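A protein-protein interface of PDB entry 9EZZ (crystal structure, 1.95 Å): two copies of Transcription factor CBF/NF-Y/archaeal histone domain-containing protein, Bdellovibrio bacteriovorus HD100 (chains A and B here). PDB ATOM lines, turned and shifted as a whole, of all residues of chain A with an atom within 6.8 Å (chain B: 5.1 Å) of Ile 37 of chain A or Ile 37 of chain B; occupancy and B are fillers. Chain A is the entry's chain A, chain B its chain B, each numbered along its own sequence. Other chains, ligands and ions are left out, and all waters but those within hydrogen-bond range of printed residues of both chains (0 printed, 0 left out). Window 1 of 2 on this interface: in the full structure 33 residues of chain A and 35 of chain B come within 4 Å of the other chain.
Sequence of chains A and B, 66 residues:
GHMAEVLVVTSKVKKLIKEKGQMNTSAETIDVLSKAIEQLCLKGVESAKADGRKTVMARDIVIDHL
Among the printed residues, merely in contact across the chains: Leu 7 of chain A with Val 8 of chain B, Val 8 of chain A with Leu 7 of chain B, Val 8 of chain A with Ile 37 of chain B, Val 13 of chain A with Cys 41 of chain B, Leu 16 of chain A with Cys 41 of chain B, Leu 33 of chain A with Leu 40 of chain B, Ala 36 of chain A with Leu 40 of chain B, Ile 37 of chain A with Val 8 of chain B, Ile 37 of chain A with Leu 33 of chain B, Ile 37 of chain A with Ile 37 of chain B, Leu 40 of chain A with Leu 33 of chain B, Leu 40 of chain A with Ala 36 of chain B, Cys 41 of chain A with Val 13 of chain B and Cys 41 of chain A with Leu 33 of chain B.
The backbone NH (N) of Leu 7 of chain A sits at hydrogen-bond distance from the side-chain hydroxyl (OG) of Ser 34 of chain A. SG of Cys 41 of chain A sits at hydrogen-bond distance from O of Ile 37 of chain A (3.4 Å). The side-chain hydroxyl of Ser 34 of chain B sits at hydrogen-bond distance from the backbone NH of Leu 7 of chain B (3.1 Å). The side-chain sulfur (SG) of Cys 41 of chain B lies within hydrogen-bond range of the backbone carbonyl oxygen (O) of Ile 37 of chain B (3.3 Å).
Val 13 of chain A touches Cys 41 of chain B, and with the chains exchanged Cys 41 of chain A touches Val 13 of chain B. Ala 36 of chain A touches Leu 40 of chain B, and with the chains exchanged Leu 40 of chain A touches Ala 36 of chain B. Ile 37 of chain A touches Leu 33 of chain B, but with the chains exchanged Leu 33 of chain A does not touch Ile 37 of chain B (4.1 Å). Cys 41 of chain A touches Leu 33 of chain B, but with the chains exchanged Leu 33 of chain A does not touch Cys 41 of chain B (4.03 Å). 13 positions are printed for both chains.
Printed residues of chain B within 4 Å of Ile 37 of chain A: Val 8, Leu 33 and Ile 37. Ile 37 of chain B touches two residues of chain A. Printed residues of chain A within 4 Å of Ala 36 of chain B: Leu 40. Printed residues of chain B within 4 Å of Leu 40 of chain A: Leu 33 and Ala 36. Ser 34 of chain B touches none of the printed residues of chain A. Ser 34 of chain A touches none of the printed residues of chain B. The nearest printed residue of chain B that does not touch Cys 41 of chain A is Val 8 of chain B (7.3 Å).
Of the 15 printed residues of chain A, 9 touch a printed residue of chain B. Hydrophobic or aromatic side chains of chain A within 4 Å of the printed part of chain B: Val 8, Val 13, Leu 16, Leu 33, Ala 36, Ile 37 and Leu 40. Hydrophobic or aromatic side chains of chain B within 4 Å of the printed part of chain A: Val 8, Val 13, Leu 33, Ala 36, Ile 37 and Leu 40.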
ATOM      1  N   LEU A   7      20.903  -3.577 -16.681  1.00  0.00           N
ATOM      2  CA  LEU A   7      22.343  -3.247 -16.892  1.00  0.00           C
ATOM      3  C   LEU A   7      23.112  -4.417 -17.521  1.00  0.00           C
ATOM      4  O   LEU A   7      24.322  -4.244 -17.782  1.00  0.00           O
ATOM      5  CB  LEU A   7      22.978  -2.865 -15.552  1.00  0.00           C
ATOM      6  CG  LEU A   7      22.418  -1.609 -14.893  1.00  0.00           C
ATOM      7  CD1 LEU A   7      23.038  -1.421 -13.521  1.00  0.00           C
ATOM      8  CD2 LEU A   7      22.674  -0.388 -15.754  1.00  0.00           C
ATOM      9  N   VAL A   8      22.471  -5.568 -17.734  1.00  0.00           N
ATOM     10  CA  VAL A   8      23.106  -6.744 -18.403  1.00  0.00           C
ATOM     11  C   VAL A   8      22.485  -6.904 -19.795  1.00  0.00           C
ATOM     12  O   VAL A   8      21.346  -6.444 -19.997  1.00  0.00           O
ATOM     13  CB  VAL A   8      22.980  -8.033 -17.571  1.00  0.00           C
ATOM     14  CG1 VAL A   8      23.582  -7.873 -16.188  1.00  0.00           C
ATOM     15  CG2 VAL A   8      21.539  -8.515 -17.471  1.00  0.00           C
ATOM     16  N   VAL A  13      23.458 -13.113 -21.824  1.00  0.00           N
ATOM     17  CA  VAL A  13      23.330 -13.844 -20.526  1.00  0.00           C
ATOM     18  C   VAL A  13      22.555 -15.148 -20.759  1.00  0.00           C
ATOM     19  O   VAL A  13      22.974 -16.199 -20.239  1.00  0.00           O
ATOM     20  CB  VAL A  13      22.649 -12.975 -19.450  1.00  0.00           C
ATOM     21  CG1 VAL A  13      22.252 -13.793 -18.234  1.00  0.00           C
ATOM     22  CG2 VAL A  13      23.522 -11.807 -19.045  1.00  0.00           C
ATOM     23  N   LEU A  16      24.781 -17.622 -22.741  1.00  0.00           N
ATOM     24  CA  LEU A  16      25.821 -18.170 -21.830  1.00  0.00           C
ATOM     25  C   LEU A  16      25.226 -19.314 -21.007  1.00  0.00           C
ATOM     26  O   LEU A  16      25.823 -20.400 -20.974  1.00  0.00           O
ATOM     27  CB  LEU A  16      26.327 -17.061 -20.904  1.00  0.00           C
ATOM     28  CG  LEU A  16      27.341 -17.518 -19.858  1.00  0.00           C
ATOM     29  CD1 LEU A  16      28.645 -17.927 -20.528  1.00  0.00           C
ATOM     30  CD2 LEU A  16      27.595 -16.436 -18.827  1.00  0.00           C
ATOM     31  N   VAL A  32      18.048  -9.590 -10.798  1.00  0.00           N
ATOM     32  CA  VAL A  32      19.042  -9.781  -9.700  1.00  0.00           C
ATOM     33  C   VAL A  32      20.446  -9.478 -10.239  1.00  0.00           C
ATOM     34  O   VAL A  32      21.196  -8.805  -9.520  1.00  0.00           O
ATOM     35  CB  VAL A  32      18.971 -11.176  -9.062  1.00  0.00           C
ATOM     36  CG1 VAL A  32      20.037 -11.353  -7.994  1.00  0.00           C
ATOM     37  CG2 VAL A  32      17.601 -11.436  -8.472  1.00  0.00           C
ATOM     38  N   LEU A  33      20.790  -9.946 -11.446  1.00  0.00           N
ATOM     39  CA  LEU A  33      22.120  -9.680 -12.057  1.00  0.00           C
ATOM     40  C   LEU A  33      22.294  -8.170 -12.241  1.00  0.00           C
ATOM     41  O   LEU A  33      23.403  -7.688 -12.004  1.00  0.00           O
ATOM     42  CB  LEU A  33      22.275 -10.413 -13.391  1.00  0.00           C
ATOM     43  CG  LEU A  33      22.429 -11.929 -13.306  1.00  0.00           C
ATOM     44  CD1 LEU A  33      22.248 -12.567 -14.684  1.00  0.00           C
ATOM     45  CD2 LEU A  33      23.772 -12.307 -12.711  1.00  0.00           C
ATOM     46  N   SER A  34      21.245  -7.461 -12.649  1.00  0.00           N
ATOM     47  CA  SER A  34      21.269  -5.989 -12.849  1.00  0.00           C
ATOM     48  C   SER A  34      21.472  -5.281 -11.505  1.00  0.00           C
ATOM     49  O   SER A  34      22.266  -4.324 -11.475  1.00  0.00           O
ATOM     50  CB  SER A  34      20.029  -5.510 -13.554  1.00  0.00           C
ATOM     51  OG  SER A  34      20.029  -5.959 -14.897  1.00  0.00           O
ATOM     52  N   LYS A  35      20.815  -5.753 -10.441  1.00  0.00           N
ATOM     53  CA  LYS A  35      21.009  -5.208  -9.067  1.00  0.00           C
ATOM     54  C   LYS A  35      22.465  -5.430  -8.646  1.00  0.00           C
ATOM     55  O   LYS A  35      23.050  -4.510  -8.062  1.00  0.00           O
ATOM     56  CB  LYS A  35      20.040  -5.838  -8.062  1.00  0.00           C
ATOM     57  N   ALA A  36      23.043  -6.596  -8.966  1.00  0.00           N
ATOM     58  CA  ALA A  36      24.442  -6.941  -8.635  1.00  0.00           C
ATOM     59  C   ALA A  36      25.367  -5.924  -9.297  1.00  0.00           C
ATOM     60  O   ALA A  36      26.269  -5.417  -8.621  1.00  0.00           O
ATOM     61  CB  ALA A  36      24.773  -8.348  -9.055  1.00  0.00           C
ATOM     62  N   ILE A  37      25.148  -5.638 -10.576  1.00  0.00           N
ATOM     63  CA  ILE A  37      25.978  -4.662 -11.340  1.00  0.00           C
ATOM     64  C   ILE A  37      25.843  -3.283 -10.691  1.00  0.00           C
ATOM     65  O   ILE A  37      26.865  -2.635 -10.484  1.00  0.00           O
ATOM     66  CB  ILE A  37      25.595  -4.629 -12.833  1.00  0.00           C
ATOM     67  CG1 ILE A  37      25.895  -5.957 -13.529  1.00  0.00           C
ATOM     68  CG2 ILE A  37      26.284  -3.481 -13.548  1.00  0.00           C
ATOM     69  CD1 ILE A  37      27.291  -6.470 -13.303  1.00  0.00           C
ATOM     70  N   GLU A  38      24.625  -2.839 -10.407  1.00  0.00           N
ATOM     71  CA  GLU A  38      24.389  -1.512  -9.788  1.00  0.00           C
ATOM     72  C   GLU A  38      25.213  -1.428  -8.499  1.00  0.00           C
ATOM     73  O   GLU A  38      25.937  -0.445  -8.347  1.00  0.00           O
ATOM     74  CB  GLU A  38      22.908  -1.273  -9.507  1.00  0.00           C
ATOM     75  CG  GLU A  38      22.649   0.126  -9.005  1.00  0.00           C
ATOM     76  CD  GLU A  38      21.242   0.363  -8.506  1.00  0.00           C
ATOM     77  OE1 GLU A  38      20.417  -0.572  -8.581  1.00  0.00           O
ATOM     78  OE2 GLU A  38      20.960   1.489  -8.065  1.00  0.00           O
ATOM     79  N   GLN A  39      25.127  -2.437  -7.630  1.00  0.00           N
ATOM     80  CA  GLN A  39      25.822  -2.423  -6.321  1.00  0.00           C
ATOM     81  C   GLN A  39      27.337  -2.366  -6.543  1.00  0.00           C
ATOM     82  O   GLN A  39      27.979  -1.588  -5.826  1.00  0.00           O
ATOM     83  CB  GLN A  39      25.413  -3.616  -5.458  1.00  0.00           C
ATOM     84  CG  GLN A  39      24.009  -3.495  -4.884  1.00  0.00           C
ATOM     85  CD  GLN A  39      23.745  -2.134  -4.284  1.00  0.00           C
ATOM     86  OE1 GLN A  39      22.942  -1.358  -4.796  1.00  0.00           O
ATOM     87  NE2 GLN A  39      24.431  -1.826  -3.194  1.00  0.00           N
ATOM     88  N   LEU A  40      27.863  -3.141  -7.505  1.00  0.00           N
ATOM     89  CA  LEU A  40      29.313  -3.165  -7.811  1.00  0.00           C
ATOM     90  C   LEU A  40      29.765  -1.780  -8.289  1.00  0.00           C
ATOM     91  O   LEU A  40      30.842  -1.331  -7.838  1.00  0.00           O
ATOM     92  CB  LEU A  40      29.620  -4.246  -8.850  1.00  0.00           C
ATOM     93  CG  LEU A  40      29.631  -5.679  -8.324  1.00  0.00           C
ATOM     94  CD1 LEU A  40      29.913  -6.657  -9.455  1.00  0.00           C
ATOM     95  CD2 LEU A  40      30.651  -5.843  -7.208  1.00  0.00           C
ATOM     96  N   CYS A  41      28.990  -1.133  -9.161  1.00  0.00           N
ATOM     97  CA  CYS A  41      29.314   0.207  -9.714  1.00  0.00           C
ATOM     98  C   CYS A  41      29.322   1.265  -8.608  1.00  0.00           C
ATOM     99  O   CYS A  41      30.203   2.132  -8.634  1.00  0.00           O
ATOM    100  CB  CYS A  41      28.302   0.629 -10.763  1.00  0.00           C
ATOM    101  SG  CYS A  41      28.490  -0.321 -12.286  1.00  0.00           S
ATOM    102  N   LEU A  42      28.347   1.212  -7.700  1.00  0.00           N
ATOM    103  CA  LEU A  42      28.217   2.203  -6.609  1.00  0.00           C
ATOM    104  C   LEU A  42      29.352   1.996  -5.600  1.00  0.00           C
ATOM    105  O   LEU A  42      29.906   2.998  -5.170  1.00  0.00           O
ATOM    106  CB  LEU A  42      26.833   2.084  -5.973  1.00  0.00           C
ATOM    107  CG  LEU A  42      25.675   2.498  -6.887  1.00  0.00           C
ATOM    108  CD1 LEU A  42      24.345   2.331  -6.175  1.00  0.00           C
ATOM    109  CD2 LEU A  42      25.840   3.938  -7.375  1.00  0.00           C
ATOM    110  N   LEU B   7      29.066  -8.497 -21.345  1.00  0.00           N
ATOM    111  CA  LEU B   7      27.755  -8.963 -20.815  1.00  0.00           C
ATOM    112  C   LEU B   7      26.998  -7.833 -20.105  1.00  0.00           C
ATOM    113  O   LEU B   7      25.873  -8.093 -19.674  1.00  0.00           O
ATOM    114  CB  LEU B   7      27.986 -10.136 -19.862  1.00  0.00           C
ATOM    115  CG  LEU B   7      28.583 -11.382 -20.503  1.00  0.00           C
ATOM    116  CD1 LEU B   7      28.942 -12.411 -19.444  1.00  0.00           C
ATOM    117  CD2 LEU B   7      27.635 -11.969 -21.536  1.00  0.00           C
ATOM    118  N   VAL B   8      27.581  -6.637 -19.977  1.00  0.00           N
ATOM    119  CA  VAL B   8      26.904  -5.459 -19.362  1.00  0.00           C
ATOM    120  C   VAL B   8      26.611  -4.449 -20.466  1.00  0.00           C
ATOM    121  O   VAL B   8      27.315  -4.461 -21.502  1.00  0.00           O
ATOM    122  CB  VAL B   8      27.712  -4.812 -18.217  1.00  0.00           C
ATOM    123  CG1 VAL B   8      27.934  -5.792 -17.091  1.00  0.00           C
ATOM    124  CG2 VAL B   8      29.020  -4.217 -18.703  1.00  0.00           C
ATOM    125  N   VAL B  13      25.806   1.545 -17.796  1.00  0.00           N
ATOM    126  CA  VAL B  13      26.798   1.469 -16.687  1.00  0.00           C
ATOM    127  C   VAL B  13      27.511   2.821 -16.579  1.00  0.00           C
ATOM    128  O   VAL B  13      27.654   3.329 -15.442  1.00  0.00           O
ATOM    129  CB  VAL B  13      27.808   0.324 -16.899  1.00  0.00           C
ATOM    130  CG1 VAL B  13      29.001   0.441 -15.961  1.00  0.00           C
ATOM    131  CG2 VAL B  13      27.151  -1.039 -16.755  1.00  0.00           C
ATOM    132  N   LEU B  33      33.285  -6.105 -14.741  1.00  0.00           N
ATOM    133  CA  LEU B  33      31.830  -6.262 -14.490  1.00  0.00           C
ATOM    134  C   LEU B  33      31.313  -7.440 -15.326  1.00  0.00           C
ATOM    135  O   LEU B  33      30.462  -8.187 -14.817  1.00  0.00           O
ATOM    136  CB  LEU B  33      31.087  -4.967 -14.816  1.00  0.00           C
ATOM    137  CG  LEU B  33      31.291  -3.805 -13.841  1.00  0.00           C
ATOM    138  CD1 LEU B  33      30.696  -2.523 -14.393  1.00  0.00           C
ATOM    139  CD2 LEU B  33      30.715  -4.100 -12.468  1.00  0.00           C
ATOM    140  N   SER B  34      31.816  -7.618 -16.550  1.00  0.00           N
ATOM    141  CA  SER B  34      31.417  -8.733 -17.442  1.00  0.00           C
ATOM    142  C   SER B  34      31.894 -10.068 -16.849  1.00  0.00           C
ATOM    143  O   SER B  34      31.123 -11.053 -16.891  1.00  0.00           O
ATOM    144  CB  SER B  34      31.905  -8.515 -18.844  1.00  0.00           C
ATOM    145  OG  SER B  34      31.219  -7.416 -19.428  1.00  0.00           O
ATOM    146  N   LYS B  35      33.113 -10.108 -16.300  1.00  0.00           N
ATOM    147  CA  LYS B  35      33.646 -11.317 -15.609  1.00  0.00           C
ATOM    148  C   LYS B  35      32.771 -11.631 -14.387  1.00  0.00           C
ATOM    149  O   LYS B  35      32.492 -12.819 -14.150  1.00  0.00           O
ATOM    150  CB  LYS B  35      35.111 -11.125 -15.217  1.00  0.00           C
ATOM    151  CG  LYS B  35      36.073 -10.981 -16.389  1.00  0.00           C
ATOM    152  CD  LYS B  35      36.414 -12.282 -17.061  1.00  0.00           C
ATOM    153  CE  LYS B  35      37.155 -12.067 -18.361  1.00  0.00           C
ATOM    154  NZ  LYS B  35      37.375 -13.356 -19.048  1.00  0.00           N
ATOM    155  N   ALA B  36      32.319 -10.605 -13.663  1.00  0.00           N
ATOM    156  CA  ALA B  36      31.437 -10.749 -12.481  1.00  0.00           C
ATOM    157  C   ALA B  36      30.146 -11.448 -12.907  1.00  0.00           C
ATOM    158  O   ALA B  36      29.736 -12.394 -12.222  1.00  0.00           O
ATOM    159  CB  ALA B  36      31.130  -9.410 -11.858  1.00  0.00           C
ATOM    160  N   ILE B  37      29.538 -10.998 -14.004  1.00  0.00           N
ATOM    161  CA  ILE B  37      28.285 -11.599 -14.549  1.00  0.00           C
ATOM    162  C   ILE B  37      28.549 -13.067 -14.879  1.00  0.00           C
ATOM    163  O   ILE B  37      27.720 -13.923 -14.493  1.00  0.00           O
ATOM    164  CB  ILE B  37      27.782 -10.832 -15.786  1.00  0.00           C
ATOM    165  CG1 ILE B  37      27.355  -9.407 -15.440  1.00  0.00           C
ATOM    166  CG2 ILE B  37      26.654 -11.602 -16.482  1.00  0.00           C
ATOM    167  CD1 ILE B  37      26.374  -9.346 -14.303  1.00  0.00           C
ATOM    168  N   GLU B  38      29.623 -13.352 -15.621  1.00  0.00           N
ATOM    169  CA  GLU B  38      29.919 -14.734 -16.046  1.00  0.00           C
ATOM    170  C   GLU B  38      29.978 -15.621 -14.801  1.00  0.00           C
ATOM    171  O   GLU B  38      29.308 -16.672 -14.787  1.00  0.00           O
ATOM    172  CB  GLU B  38      31.200 -14.764 -16.864  1.00  0.00           C
ATOM    173  CG  GLU B  38      31.632 -16.164 -17.248  1.00  0.00           C
ATOM    174  CD  GLU B  38      32.787 -16.163 -18.224  1.00  0.00           C
ATOM    175  OE1 GLU B  38      33.464 -15.112 -18.324  1.00  0.00           O
ATOM    176  OE2 GLU B  38      33.006 -17.201 -18.878  1.00  0.00           O
ATOM    177  N   GLN B  39      30.709 -15.190 -13.771  1.00  0.00           N
ATOM    178  CA  GLN B  39      30.913 -16.002 -12.546  1.00  0.00           C
ATOM    179  C   GLN B  39      29.569 -16.217 -11.845  1.00  0.00           C
ATOM    180  O   GLN B  39      29.326 -17.344 -11.393  1.00  0.00           O
ATOM    181  CB  GLN B  39      31.949 -15.364 -11.619  1.00  0.00           C
ATOM    182  CG  GLN B  39      33.380 -15.509 -12.135  1.00  0.00           C
ATOM    183  CD  GLN B  39      33.699 -16.881 -12.696  1.00  0.00           C
ATOM    184  OE1 GLN B  39      33.725 -17.884 -11.982  1.00  0.00           O
ATOM    185  NE2 GLN B  39      33.945 -16.946 -13.998  1.00  0.00           N
ATOM    186  N   LEU B  40      28.737 -15.173 -11.754  1.00  0.00           N
ATOM    187  CA  LEU B  40      27.405 -15.263 -11.100  1.00  0.00           C
ATOM    188  C   LEU B  40      26.513 -16.257 -11.855  1.00  0.00           C
ATOM    189  O   LEU B  40      25.818 -17.031 -11.183  1.00  0.00           O
ATOM    190  CB  LEU B  40      26.751 -13.877 -11.045  1.00  0.00           C
ATOM    191  CG  LEU B  40      27.263 -12.942  -9.954  1.00  0.00           C
ATOM    192  CD1 LEU B  40      26.494 -11.631  -9.990  1.00  0.00           C
ATOM    193  CD2 LEU B  40      27.161 -13.577  -8.576  1.00  0.00           C
ATOM    194  N   CYS B  41      26.533 -16.248 -13.189  1.00  0.00           N
ATOM    195  CA  CYS B  41      25.723 -17.171 -14.029  1.00  0.00           C
ATOM    196  C   CYS B  41      26.166 -18.620 -13.830  1.00  0.00           C
ATOM    197  O   CYS B  41      25.298 -19.487 -13.760  1.00  0.00           O
ATOM    198  CB  CYS B  41      25.822 -16.828 -15.505  1.00  0.00           C
ATOM    199  SG  CYS B  41      24.982 -15.274 -15.867  1.00  0.00           S
ATOM    200  N   LEU B  42      27.469 -18.861 -13.768  1.00  0.00           N
ATOM    201  CA  LEU B  42      28.043 -20.220 -13.596  1.00  0.00           C
ATOM    202  C   LEU B  42      27.711 -20.742 -12.188  1.00  0.00           C
ATOM    203  O   LEU B  42      27.301 -21.916 -12.099  1.00  0.00           O
ATOM    204  CB  LEU B  42      29.547 -20.170 -13.871  1.00  0.00           C
ATOM    205  CG  LEU B  42      29.919 -19.871 -15.325  1.00  0.00           C
ATOM    206  CD1 LEU B  42      31.429 -19.779 -15.498  1.00  0.00           C
ATOM    207  CD2 LEU B  42      29.335 -20.910 -16.275  1.00  0.00           C
